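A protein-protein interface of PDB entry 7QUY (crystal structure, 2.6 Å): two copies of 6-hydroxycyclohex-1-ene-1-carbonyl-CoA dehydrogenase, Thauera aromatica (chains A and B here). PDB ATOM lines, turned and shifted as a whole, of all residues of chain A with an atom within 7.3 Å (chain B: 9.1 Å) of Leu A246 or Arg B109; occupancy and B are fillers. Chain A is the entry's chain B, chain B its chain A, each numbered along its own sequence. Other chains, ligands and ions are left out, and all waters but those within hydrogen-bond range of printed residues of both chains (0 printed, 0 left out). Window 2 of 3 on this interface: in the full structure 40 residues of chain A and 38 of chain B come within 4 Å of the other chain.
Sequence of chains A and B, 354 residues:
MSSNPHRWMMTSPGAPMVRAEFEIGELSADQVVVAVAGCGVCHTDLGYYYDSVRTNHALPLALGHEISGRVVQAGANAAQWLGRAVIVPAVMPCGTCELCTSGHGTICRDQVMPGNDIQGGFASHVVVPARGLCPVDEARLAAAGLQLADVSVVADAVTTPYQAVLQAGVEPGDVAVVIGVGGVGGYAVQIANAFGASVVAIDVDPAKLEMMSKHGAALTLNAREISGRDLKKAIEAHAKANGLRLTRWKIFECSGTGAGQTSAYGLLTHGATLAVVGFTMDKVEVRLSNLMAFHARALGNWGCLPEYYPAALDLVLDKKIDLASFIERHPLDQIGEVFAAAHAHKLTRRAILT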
ATOM      1  N   GLY A 173       2.813   4.711  30.332  1.00  0.00           N
ATOM      2  CA  GLY A 173       3.729   5.863  30.348  1.00  0.00           C
ATOM      3  C   GLY A 173       3.527   6.732  29.128  1.00  0.00           C
ATOM      4  O   GLY A 173       4.004   7.885  29.155  1.00  0.00           O
ATOM      5  N   VAL A 175       1.852   9.278  26.509  1.00  0.00           N
ATOM      6  CA  VAL A 175       0.811  10.272  26.134  1.00  0.00           C
ATOM      7  C   VAL A 175       0.126   9.744  24.874  1.00  0.00           C
ATOM      8  O   VAL A 175       0.847   9.387  23.928  1.00  0.00           O
ATOM      9  CB  VAL A 175       1.406  11.664  25.869  1.00  0.00           C
ATOM     10  CG1 VAL A 175       0.347  12.638  25.377  1.00  0.00           C
ATOM     11  CG2 VAL A 175       2.121  12.205  27.097  1.00  0.00           C
ATOM     12  N   ILE A 235       0.279  20.056  25.776  1.00  0.00           N
ATOM     13  CA  ILE A 235       0.443  18.577  25.909  1.00  0.00           C
ATOM     14  C   ILE A 235       1.830  18.297  26.497  1.00  0.00           C
ATOM     15  O   ILE A 235       1.926  17.405  27.366  1.00  0.00           O
ATOM     16  CB  ILE A 235       0.163  17.849  24.580  1.00  0.00           C
ATOM     17  CG1 ILE A 235      -1.282  18.081  24.125  1.00  0.00           C
ATOM     18  CG2 ILE A 235       0.448  16.360  24.708  1.00  0.00           C
ATOM     19  CD1 ILE A 235      -1.508  17.821  22.666  1.00  0.00           C
ATOM     20  N   GLU A 236       2.849  19.054  26.079  1.00  0.00           N
ATOM     21  CA  GLU A 236       4.209  19.032  26.692  1.00  0.00           C
ATOM     22  C   GLU A 236       4.038  19.268  28.197  1.00  0.00           C
ATOM     23  O   GLU A 236       4.584  18.469  28.991  1.00  0.00           O
ATOM     24  CB  GLU A 236       5.148  20.056  26.027  1.00  0.00           C
ATOM     25  CG  GLU A 236       5.577  19.650  24.619  1.00  0.00           C
ATOM     26  CD  GLU A 236       6.625  20.497  23.908  1.00  0.00           C
ATOM     27  OE1 GLU A 236       6.849  21.649  24.321  1.00  0.00           O
ATOM     28  OE2 GLU A 236       7.235  19.987  22.937  1.00  0.00           O
ATOM     29  N   ALA A 237       3.260  20.294  28.560  1.00  0.00           N
ATOM     30  CA  ALA A 237       2.942  20.676  29.958  1.00  0.00           C
ATOM     31  C   ALA A 237       2.322  19.483  30.682  1.00  0.00           C
ATOM     32  O   ALA A 237       2.813  19.140  31.767  1.00  0.00           O
ATOM     33  CB  ALA A 237       2.021  21.873  29.989  1.00  0.00           C
ATOM     34  N   HIS A 238       1.294  18.871  30.095  1.00  0.00           N
ATOM     35  CA  HIS A 238       0.580  17.715  30.694  1.00  0.00           C
ATOM     36  C   HIS A 238       1.584  16.590  30.978  1.00  0.00           C
ATOM     37  O   HIS A 238       1.525  16.004  32.087  1.00  0.00           O
ATOM     38  CB  HIS A 238      -0.595  17.272  29.811  1.00  0.00           C
ATOM     39  CG  HIS A 238      -1.223  16.000  30.271  1.00  0.00           C
ATOM     40  ND1 HIS A 238      -2.086  15.946  31.338  1.00  0.00           N
ATOM     41  CD2 HIS A 238      -1.091  14.732  29.816  1.00  0.00           C
ATOM     42  CE1 HIS A 238      -2.464  14.696  31.525  1.00  0.00           C
ATOM     43  NE2 HIS A 238      -1.871  13.930  30.599  1.00  0.00           N
ATOM     44  N   ALA A 239       2.482  16.324  30.030  1.00  0.00           N
ATOM     45  CA  ALA A 239       3.458  15.213  30.094  1.00  0.00           C
ATOM     46  C   ALA A 239       4.474  15.474  31.210  1.00  0.00           C
ATOM     47  O   ALA A 239       4.719  14.532  32.012  1.00  0.00           O
ATOM     48  CB  ALA A 239       4.156  15.064  28.770  1.00  0.00           C
ATOM     49  N   LYS A 240       5.042  16.692  31.229  1.00  0.00           N
ATOM     50  CA  LYS A 240       6.089  17.142  32.182  1.00  0.00           C
ATOM     51  C   LYS A 240       5.519  17.071  33.602  1.00  0.00           C
ATOM     52  O   LYS A 240       6.153  16.424  34.461  1.00  0.00           O
ATOM     53  CB  LYS A 240       6.552  18.567  31.861  1.00  0.00           C
ATOM     54  CG  LYS A 240       7.526  18.721  30.695  1.00  0.00           C
ATOM     55  CD  LYS A 240       8.579  19.805  30.930  1.00  0.00           C
ATOM     56  CE  LYS A 240       8.839  20.694  29.731  1.00  0.00           C
ATOM     57  NZ  LYS A 240       7.719  21.643  29.513  1.00  0.00           N
ATOM     58  N   GLY A 243       4.973  13.331  34.753  1.00  0.00           N
ATOM     59  CA  GLY A 243       6.109  12.406  34.578  1.00  0.00           C
ATOM     60  C   GLY A 243       5.837  11.408  33.473  1.00  0.00           C
ATOM     61  O   GLY A 243       6.142  10.225  33.654  1.00  0.00           O
ATOM     62  N   LEU A 244       5.260  11.887  32.371  1.00  0.00           N
ATOM     63  CA  LEU A 244       4.898  11.066  31.193  1.00  0.00           C
ATOM     64  C   LEU A 244       5.953  11.282  30.105  1.00  0.00           C
ATOM     65  O   LEU A 244       6.678  12.299  30.155  1.00  0.00           O
ATOM     66  CB  LEU A 244       3.517  11.487  30.683  1.00  0.00           C
ATOM     67  CG  LEU A 244       2.356  11.278  31.654  1.00  0.00           C
ATOM     68  CD1 LEU A 244       1.113  12.017  31.174  1.00  0.00           C
ATOM     69  CD2 LEU A 244       2.058   9.798  31.865  1.00  0.00           C
ATOM     70  N   ARG A 245       5.988  10.368  29.137  1.00  0.00           N
ATOM     71  CA  ARG A 245       6.934  10.367  27.998  1.00  0.00           C
ATOM     72  C   ARG A 245       6.825  11.685  27.209  1.00  0.00           C
ATOM     73  O   ARG A 245       5.693  12.085  26.903  1.00  0.00           O
ATOM     74  CB  ARG A 245       6.637   9.122  27.163  1.00  0.00           C
ATOM     75  CG  ARG A 245       7.512   7.943  27.546  1.00  0.00           C
ATOM     76  CD  ARG A 245       6.867   6.614  27.843  1.00  0.00           C
ATOM     77  NE  ARG A 245       6.619   5.867  26.618  1.00  0.00           N
ATOM     78  CZ  ARG A 245       6.824   4.562  26.441  1.00  0.00           C
ATOM     79  NH1 ARG A 245       7.323   3.816  27.405  1.00  0.00           N
ATOM     80  NH2 ARG A 245       6.531   4.002  25.281  1.00  0.00           N
ATOM     81  N   LEU A 246       7.959  12.342  26.911  1.00  0.00           N
ATOM     82  CA  LEU A 246       8.052  13.467  25.947  1.00  0.00           C
ATOM     83  C   LEU A 246       8.301  12.927  24.527  1.00  0.00           C
ATOM     84  O   LEU A 246       8.283  13.747  23.569  1.00  0.00           O
ATOM     85  CB  LEU A 246       9.177  14.422  26.358  1.00  0.00           C
ATOM     86  CG  LEU A 246       8.813  15.596  27.266  1.00  0.00           C
ATOM     87  CD1 LEU A 246       7.351  15.982  27.157  1.00  0.00           C
ATOM     88  CD2 LEU A 246       9.167  15.293  28.710  1.00  0.00           C
ATOM     89  N   THR A 247       8.523  11.614  24.399  1.00  0.00           N
ATOM     90  CA  THR A 247       8.734  10.907  23.109  1.00  0.00           C
ATOM     91  C   THR A 247       7.601   9.904  22.885  1.00  0.00           C
ATOM     92  O   THR A 247       6.837   9.642  23.840  1.00  0.00           O
ATOM     93  CB  THR A 247      10.104  10.216  23.063  1.00  0.00           C
ATOM     94  OG1 THR A 247      10.146   9.112  23.973  1.00  0.00           O
ATOM     95  CG2 THR A 247      11.220  11.192  23.355  1.00  0.00           C
ATOM     96  N   ARG A 248       7.483   9.396  21.656  1.00  0.00           N
ATOM     97  CA  ARG A 248       6.692   8.180  21.324  1.00  0.00           C
ATOM     98  C   ARG A 248       5.190   8.440  21.507  1.00  0.00           C
ATOM     99  O   ARG A 248       4.437   7.452  21.695  1.00  0.00           O
ATOM    100  CB  ARG A 248       7.214   7.029  22.183  1.00  0.00           C
ATOM    101  CG  ARG A 248       8.668   6.687  21.891  1.00  0.00           C
ATOM    102  CD  ARG A 248       9.243   5.733  22.907  1.00  0.00           C
ATOM    103  NE  ARG A 248       9.561   6.423  24.137  1.00  0.00           N
ATOM    104  CZ  ARG A 248       9.942   5.826  25.253  1.00  0.00           C
ATOM    105  NH1 ARG A 248      10.241   6.560  26.310  1.00  0.00           N
ATOM    106  NH2 ARG A 248      10.049   4.509  25.305  1.00  0.00           N
ATOM    107  N   TRP A 249       4.760   9.700  21.399  1.00  0.00           N
ATOM    108  CA  TRP A 249       3.330  10.095  21.499  1.00  0.00           C
ATOM    109  C   TRP A 249       2.512   9.281  20.496  1.00  0.00           C
ATOM    110  O   TRP A 249       2.945   9.187  19.360  1.00  0.00           O
ATOM    111  CB  TRP A 249       3.156  11.601  21.282  1.00  0.00           C
ATOM    112  CG  TRP A 249       3.629  12.457  22.419  1.00  0.00           C
ATOM    113  CD1 TRP A 249       4.237  12.063  23.581  1.00  0.00           C
ATOM    114  CD2 TRP A 249       3.586  13.894  22.467  1.00  0.00           C
ATOM    115  NE1 TRP A 249       4.553  13.154  24.348  1.00  0.00           N
ATOM    116  CE2 TRP A 249       4.189  14.289  23.679  1.00  0.00           C
ATOM    117  CE3 TRP A 249       3.089  14.879  21.606  1.00  0.00           C
ATOM    118  CZ2 TRP A 249       4.300  15.628  24.039  1.00  0.00           C
ATOM    119  CZ3 TRP A 249       3.214  16.205  21.954  1.00  0.00           C
ATOM    120  CH2 TRP A 249       3.805  16.571  23.160  1.00  0.00           C
ATOM    121  N   THR A 269       6.367  14.133  17.392  1.00  0.00           N
ATOM    122  CA  THR A 269       7.629  14.315  18.140  1.00  0.00           C
ATOM    123  C   THR A 269       8.468  13.037  17.975  1.00  0.00           C
ATOM    124  O   THR A 269       7.989  12.066  17.360  1.00  0.00           O
ATOM    125  CB  THR A 269       7.315  14.683  19.595  1.00  0.00           C
ATOM    126  OG1 THR A 269       8.450  15.357  20.152  1.00  0.00           O
ATOM    127  CG2 THR A 269       6.934  13.470  20.418  1.00  0.00           C
ATOM    128  N   HIS A 270       9.680  13.045  18.517  1.00  0.00           N
ATOM    129  CA  HIS A 270      10.665  11.939  18.403  1.00  0.00           C
ATOM    130  C   HIS A 270       9.971  10.612  18.721  1.00  0.00           C
ATOM    131  O   HIS A 270       9.410  10.498  19.822  1.00  0.00           O
ATOM    132  CB  HIS A 270      11.882  12.251  19.281  1.00  0.00           C
ATOM    133  CG  HIS A 270      12.644  13.439  18.799  1.00  0.00           C
ATOM    134  ND1 HIS A 270      12.316  14.719  19.178  1.00  0.00           N
ATOM    135  CD2 HIS A 270      13.692  13.550  17.947  1.00  0.00           C
ATOM    136  CE1 HIS A 270      13.131  15.574  18.588  1.00  0.00           C
ATOM    137  NE2 HIS A 270      13.983  14.880  17.822  1.00  0.00           N
ATOM    138  N   GLY A 271       9.930   9.696  17.752  1.00  0.00           N
ATOM    139  CA  GLY A 271       9.407   8.318  17.912  1.00  0.00           C
ATOM    140  C   GLY A 271       7.889   8.242  17.935  1.00  0.00           C
ATOM    141  O   GLY A 271       7.356   7.173  18.271  1.00  0.00           O
ATOM    142  N   ASN B  56      27.231  20.832  16.880  1.00  0.00           N
ATOM    143  CA  ASN B  56      26.964  20.748  18.342  1.00  0.00           C
ATOM    144  C   ASN B  56      28.224  21.146  19.106  1.00  0.00           C
ATOM    145  O   ASN B  56      28.087  21.859  20.121  1.00  0.00           O
ATOM    146  CB  ASN B  56      26.512  19.349  18.772  1.00  0.00           C
ATOM    147  CG  ASN B  56      25.177  18.933  18.186  1.00  0.00           C
ATOM    148  OD1 ASN B  56      24.834  17.764  18.214  1.00  0.00           O
ATOM    149  ND2 ASN B  56      24.399  19.862  17.662  1.00  0.00           N
ATOM    150  N   VAL B  91      26.841   7.684  14.006  1.00  0.00           N
ATOM    151  CA  VAL B  91      26.090   8.198  15.189  1.00  0.00           C
ATOM    152  C   VAL B  91      25.993   7.075  16.217  1.00  0.00           C
ATOM    153  O   VAL B  91      25.507   6.017  15.842  1.00  0.00           O
ATOM    154  CB  VAL B  91      24.700   8.738  14.783  1.00  0.00           C
ATOM    155  CG1 VAL B  91      23.956   9.279  15.983  1.00  0.00           C
ATOM    156  CG2 VAL B  91      24.783   9.816  13.695  1.00  0.00           C
ATOM    157  N   MET B  92      26.437   7.313  17.461  1.00  0.00           N
ATOM    158  CA  MET B  92      26.548   6.283  18.537  1.00  0.00           C
ATOM    159  C   MET B  92      25.613   6.629  19.698  1.00  0.00           C
ATOM    160  O   MET B  92      25.837   7.565  20.461  1.00  0.00           O
ATOM    161  CB  MET B  92      28.002   6.159  18.995  1.00  0.00           C
ATOM    162  CG  MET B  92      28.921   5.775  17.823  1.00  0.00           C
ATOM    163  SD  MET B  92      30.613   6.438  17.876  1.00  0.00           S
ATOM    164  CE  MET B  92      31.457   4.932  18.376  1.00  0.00           C
ATOM    165  N   PRO B  93      24.478   5.910  19.826  1.00  0.00           N
ATOM    166  CA  PRO B  93      23.595   6.043  20.985  1.00  0.00           C
ATOM    167  C   PRO B  93      24.270   5.611  22.292  1.00  0.00           C
ATOM    168  O   PRO B  93      25.193   4.844  22.187  1.00  0.00           O
ATOM    169  CB  PRO B  93      22.435   5.088  20.641  1.00  0.00           C
ATOM    170  CG  PRO B  93      22.450   4.982  19.151  1.00  0.00           C
ATOM    171  CD  PRO B  93      23.920   5.006  18.806  1.00  0.00           C
ATOM    172  N   CYS B  94      23.706   6.016  23.450  1.00  0.00           N
ATOM    173  CA  CYS B  94      24.143   5.666  24.833  1.00  0.00           C
ATOM    174  C   CYS B  94      24.269   4.186  25.053  1.00  0.00           C
ATOM    175  O   CYS B  94      25.255   3.747  25.660  1.00  0.00           O
ATOM    176  CB  CYS B  94      22.944   5.871  25.773  1.00  0.00           C
ATOM    177  SG  CYS B  94      21.643   4.573  25.815  1.00  0.00           S
ATOM    178  N   GLY B  95      23.312   3.464  24.539  1.00  0.00           N
ATOM    179  CA  GLY B  95      23.100   2.035  24.824  1.00  0.00           C
ATOM    180  C   GLY B  95      22.542   1.750  26.211  1.00  0.00           C
ATOM    181  O   GLY B  95      22.363   0.544  26.503  1.00  0.00           O
ATOM    182  N   CYS B  97      20.035   4.110  27.972  1.00  0.00           N
ATOM    183  CA  CYS B  97      18.790   4.866  28.278  1.00  0.00           C
ATOM    184  C   CYS B  97      17.539   4.089  27.853  1.00  0.00           C
ATOM    185  O   CYS B  97      17.657   3.209  26.977  1.00  0.00           O
ATOM    186  CB  CYS B  97      18.801   6.222  27.581  1.00  0.00           C
ATOM    187  SG  CYS B  97      18.289   6.149  25.845  1.00  0.00           S
ATOM    188  N   GLU B  98      16.389   4.422  28.444  1.00  0.00           N
ATOM    189  CA  GLU B  98      15.093   3.761  28.143  1.00  0.00           C
ATOM    190  C   GLU B  98      14.863   3.730  26.621  1.00  0.00           C
ATOM    191  O   GLU B  98      14.385   2.700  26.128  1.00  0.00           O
ATOM    192  CB  GLU B  98      13.958   4.475  28.881  1.00  0.00           C
ATOM    193  CG  GLU B  98      12.567   3.892  28.635  1.00  0.00           C
ATOM    194  CD  GLU B  98      11.433   4.879  28.889  1.00  0.00           C
ATOM    195  OE1 GLU B  98      11.633   6.088  28.636  1.00  0.00           O
ATOM    196  OE2 GLU B  98      10.352   4.463  29.346  1.00  0.00           O
ATOM    197  N   LEU B  99      15.190   4.801  25.896  1.00  0.00           N
ATOM    198  CA  LEU B  99      15.034   4.868  24.427  1.00  0.00           C
ATOM    199  C   LEU B  99      15.956   3.825  23.785  1.00  0.00           C
ATOM    200  O   LEU B  99      15.435   3.005  22.986  1.00  0.00           O
ATOM    201  CB  LEU B  99      15.335   6.288  23.924  1.00  0.00           C
ATOM    202  CG  LEU B  99      14.377   7.378  24.407  1.00  0.00           C
ATOM    203  CD1 LEU B  99      14.825   8.755  23.957  1.00  0.00           C
ATOM    204  CD2 LEU B  99      12.962   7.111  23.933  1.00  0.00           C
ATOM    205  N   CYS B 100      17.257   3.836  24.124  1.00  0.00           N
ATOM    206  CA  CYS B 100      18.277   2.930  23.508  1.00  0.00           C
ATOM    207  C   CYS B 100      17.837   1.467  23.865  1.00  0.00           C
ATOM    208  O   CYS B 100      17.831   0.585  22.974  1.00  0.00           O
ATOM    209  CB  CYS B 100      19.763   3.339  23.733  1.00  0.00           C
ATOM    210  SG  CYS B 100      20.509   4.985  23.577  1.00  0.00           S
ATOM    211  N   HIS B 104      14.723   2.182  20.484  1.00  0.00           N
ATOM    212  CA  HIS B 104      14.636   3.557  19.913  1.00  0.00           C
ATOM    213  C   HIS B 104      15.984   4.302  19.967  1.00  0.00           C
ATOM    214  O   HIS B 104      15.964   5.541  20.076  1.00  0.00           O
ATOM    215  CB  HIS B 104      13.552   4.356  20.638  1.00  0.00           C
ATOM    216  CG  HIS B 104      12.169   3.845  20.430  1.00  0.00           C
ATOM    217  ND1 HIS B 104      11.629   2.826  21.191  1.00  0.00           N
ATOM    218  CD2 HIS B 104      11.201   4.239  19.582  1.00  0.00           C
ATOM    219  CE1 HIS B 104      10.388   2.601  20.801  1.00  0.00           C
ATOM    220  NE2 HIS B 104      10.094   3.470  19.831  1.00  0.00           N
ATOM    221  N   GLY B 105      17.109   3.594  19.843  1.00  0.00           N
ATOM    222  CA  GLY B 105      18.465   4.172  19.742  1.00  0.00           C
ATOM    223  C   GLY B 105      18.582   5.351  18.769  1.00  0.00           C
ATOM    224  O   GLY B 105      19.396   6.263  19.036  1.00  0.00           O
ATOM    225  N   THR B 106      17.859   5.367  17.653  1.00  0.00           N
ATOM    226  CA  THR B 106      17.976   6.471  16.659  1.00  0.00           C
ATOM    227  C   THR B 106      17.564   7.810  17.289  1.00  0.00           C
ATOM    228  O   THR B 106      17.958   8.850  16.745  1.00  0.00           O
ATOM    229  CB  THR B 106      17.151   6.206  15.391  1.00  0.00           C
ATOM    230  OG1 THR B 106      15.839   5.752  15.756  1.00  0.00           O
ATOM    231  CG2 THR B 106      17.842   5.207  14.490  1.00  0.00           C
ATOM    232  N   ILE B 107      16.800   7.801  18.383  1.00  0.00           N
ATOM    233  CA  ILE B 107      16.358   9.060  19.047  1.00  0.00           C
ATOM    234  C   ILE B 107      16.938   9.165  20.467  1.00  0.00           C
ATOM    235  O   ILE B 107      16.395   9.991  21.215  1.00  0.00           O
ATOM    236  CB  ILE B 107      14.821   9.192  19.020  1.00  0.00           C
ATOM    237  CG1 ILE B 107      14.106   7.986  19.631  1.00  0.00           C
ATOM    238  CG2 ILE B 107      14.336   9.444  17.606  1.00  0.00           C
ATOM    239  CD1 ILE B 107      12.686   8.283  20.088  1.00  0.00           C
ATOM    240  N   CYS B 108      18.042   8.476  20.649  1.00  0.00           N
ATOM    241  CA  CYS B 108      18.621   8.706  21.957  1.00  0.00           C
ATOM    242  C   CYS B 108      18.939  10.167  22.056  1.00  0.00           C
ATOM    243  O   CYS B 108      19.396  10.759  21.071  1.00  0.00           O
ATOM    244  CB  CYS B 108      19.932   8.040  22.225  1.00  0.00           C
ATOM    245  SG  CYS B 108      19.603   7.534  23.907  1.00  0.00           S
ATOM    246  N   ARG B 109      18.742  10.687  23.239  1.00  0.00           N
ATOM    247  CA  ARG B 109      19.127  12.135  23.298  1.00  0.00           C
ATOM    248  C   ARG B 109      20.622  12.361  23.504  1.00  0.00           C
ATOM    249  O   ARG B 109      21.085  13.475  23.226  1.00  0.00           O
ATOM    250  CB  ARG B 109      18.363  12.804  24.440  1.00  0.00           C
ATOM    251  CG  ARG B 109      16.938  12.299  24.610  1.00  0.00           C
ATOM    252  CD  ARG B 109      16.373  12.660  25.969  1.00  0.00           C
ATOM    253  NE  ARG B 109      15.078  13.312  25.869  1.00  0.00           N
ATOM    254  CZ  ARG B 109      13.928  12.754  26.227  1.00  0.00           C
ATOM    255  NH1 ARG B 109      13.914  11.525  26.709  1.00  0.00           N
ATOM    256  NH2 ARG B 109      12.799  13.426  26.099  1.00  0.00           N
ATOM    257  N   ASP B 110      21.328  11.369  24.001  1.00  0.00           N
ATOM    258  CA  ASP B 110      22.793  11.391  24.264  1.00  0.00           C
ATOM    259  C   ASP B 110      23.569  10.633  23.189  1.00  0.00           C
ATOM    260  O   ASP B 110      24.540   9.923  23.544  1.00  0.00           O
ATOM    261  CB  ASP B 110      23.156  10.776  25.621  1.00  0.00           C
ATOM    262  CG  ASP B 110      22.345  11.332  26.773  1.00  0.00           C
ATOM    263  OD1 ASP B 110      22.467  12.543  27.022  1.00  0.00           O
ATOM    264  OD2 ASP B 110      21.577  10.551  27.400  1.00  0.00           O
ATOM    265  N   GLN B 111      23.199  10.794  21.923  1.00  0.00           N
ATOM    266  CA  GLN B 111      23.906  10.130  20.791  1.00  0.00           C
ATOM    267  C   GLN B 111      25.063  11.047  20.390  1.00  0.00           C
ATOM    268  O   GLN B 111      24.900  12.274  20.490  1.00  0.00           O
ATOM    269  CB  GLN B 111      22.957   9.797  19.630  1.00  0.00           C
ATOM    270  CG  GLN B 111      22.224  11.006  19.040  1.00  0.00           C
ATOM    271  CD  GLN B 111      21.242  10.666  17.943  1.00  0.00           C
ATOM    272  OE1 GLN B 111      21.251  11.241  16.849  1.00  0.00           O
ATOM    273  NE2 GLN B 111      20.369   9.715  18.227  1.00  0.00           N
ATOM    274  N   VAL B 112      26.198  10.473  20.002  1.00  0.00           N
ATOM    275  CA  VAL B 112      27.423  11.248  19.660  1.00  0.00           C
ATOM    276  C   VAL B 112      27.813  10.895  18.223  1.00  0.00           C
ATOM    277  O   VAL B 112      27.922   9.706  17.885  1.00  0.00           O
ATOM    278  CB  VAL B 112      28.577  11.093  20.682  1.00  0.00           C
ATOM    279  CG1 VAL B 112      28.217  10.196  21.860  1.00  0.00           C
ATOM    280  CG2 VAL B 112      29.891  10.659  20.042  1.00  0.00           C
ATOM    281  N   ASP B 117      29.467  16.319  17.121  1.00  0.00           N
ATOM    282  CA  ASP B 117      29.490  16.300  18.608  1.00  0.00           C
ATOM    283  C   ASP B 117      30.932  16.208  19.098  1.00  0.00           C
ATOM    284  O   ASP B 117      31.230  16.772  20.149  1.00  0.00           O
ATOM    285  CB  ASP B 117      28.707  15.111  19.169  1.00  0.00           C
ATOM    286  CG  ASP B 117      27.213  15.227  18.966  1.00  0.00           C
ATOM    287  OD1 ASP B 117      26.653  16.249  19.431  1.00  0.00           O
ATOM    288  OD2 ASP B 117      26.625  14.298  18.342  1.00  0.00           O
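The side-chain carboxylate of Glu B98 is in salt-bridge range of the guanidinium group of Arg A245 (3.7 Å).
OE1 of Glu B98 lies within salt-bridge range of NH1 of Arg A248 (2.8 Å).
The backbone carbonyl oxygen of Arg A245 is in hydrogen-bond range of the indole nitrogen of Trp A249, 3.0 Å away.
O of His A270 lies within hydrogen-bond range of N of Arg A248 (2.9 Å).
The backbone carbonyl oxygen (O) of Leu B99 is in hydrogen-bond range of the backbone NH (N) of His B104.
The backbone carbonyl oxygen (O) of Gly A173 lies within hydrogen-bond range of the backbone NH (N) of Arg A245.
OG1 of Thr A247 lies within hydrogen-bond range of NE of Arg A248 (2.8 Å).
The side-chain sulfur of Cys B97 lies close to the backbone NH of Leu B99 (3.4 Å).
Arg B109 touches Leu A246.
Thr A247 touches Leu B99 (OG1 to CD2, 3.5 Å).
Thr A247 touches Arg B109.
Leu B99 touches Arg A248.
CD of Arg A248 touches NE2 of His B104, at 3.9 Å.
His A270 touches Ile B107 (C to CD1, 3.8 Å).
Ile B107 touches Gly A271.
Ile A235 touches none of the printed residues of chain B.
Of the printed residues of chain B, Arg A245 touches Glu B98.
Of chain B, only Arg B109 (3.8 Å) comes within 4 Å of Leu A246.
Thr A269 touches none of the printed residues of chain B.
Of the printed residues of chain B, His A270 touches Ile B107.
Of the printed residues of chain A, Leu B99 touches Thr A247 and Arg A248.
Of the printed residues of chain A, Ile B107 touches His A270 (3.8 Å) and Gly A271 (3.9 Å).
The nearest printed residue of chain B that does not touch Leu A246 is Glu B98 (7.5 Å).
The nearest residue of chain A that does not touch Arg B109 is Arg A248 (6.2 Å).
Of the 18 printed residues of chain A, 6 touch a printed residue of chain B.
Hydrophobic or aromatic side chains of chain A within 4 Å of the printed part of chain B: Leu A246.
Of the 20 printed residues of chain B, 5 touch a printed residue of chain A.
Printed residues of chain B that touch a printed residue of chain A: Glu B98, Leu B99, His B104, Ile B107 and Arg B109.
Hydrophobic or aromatic side chains of chain B within 4 Å of the printed part of chain A: Leu B99, His B104 and Ile B107.
Among the printed residues, 9 pairs touch across the chains.
Among the printed residues, Asp or Glu carboxylates within 4 Å of a Lys or Arg side-chain nitrogen of the other chain: Arg A245 with Glu B98 (3.7 Å) and Arg A248 with Glu B98 (2.8 Å).
No position is printed for both chains.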
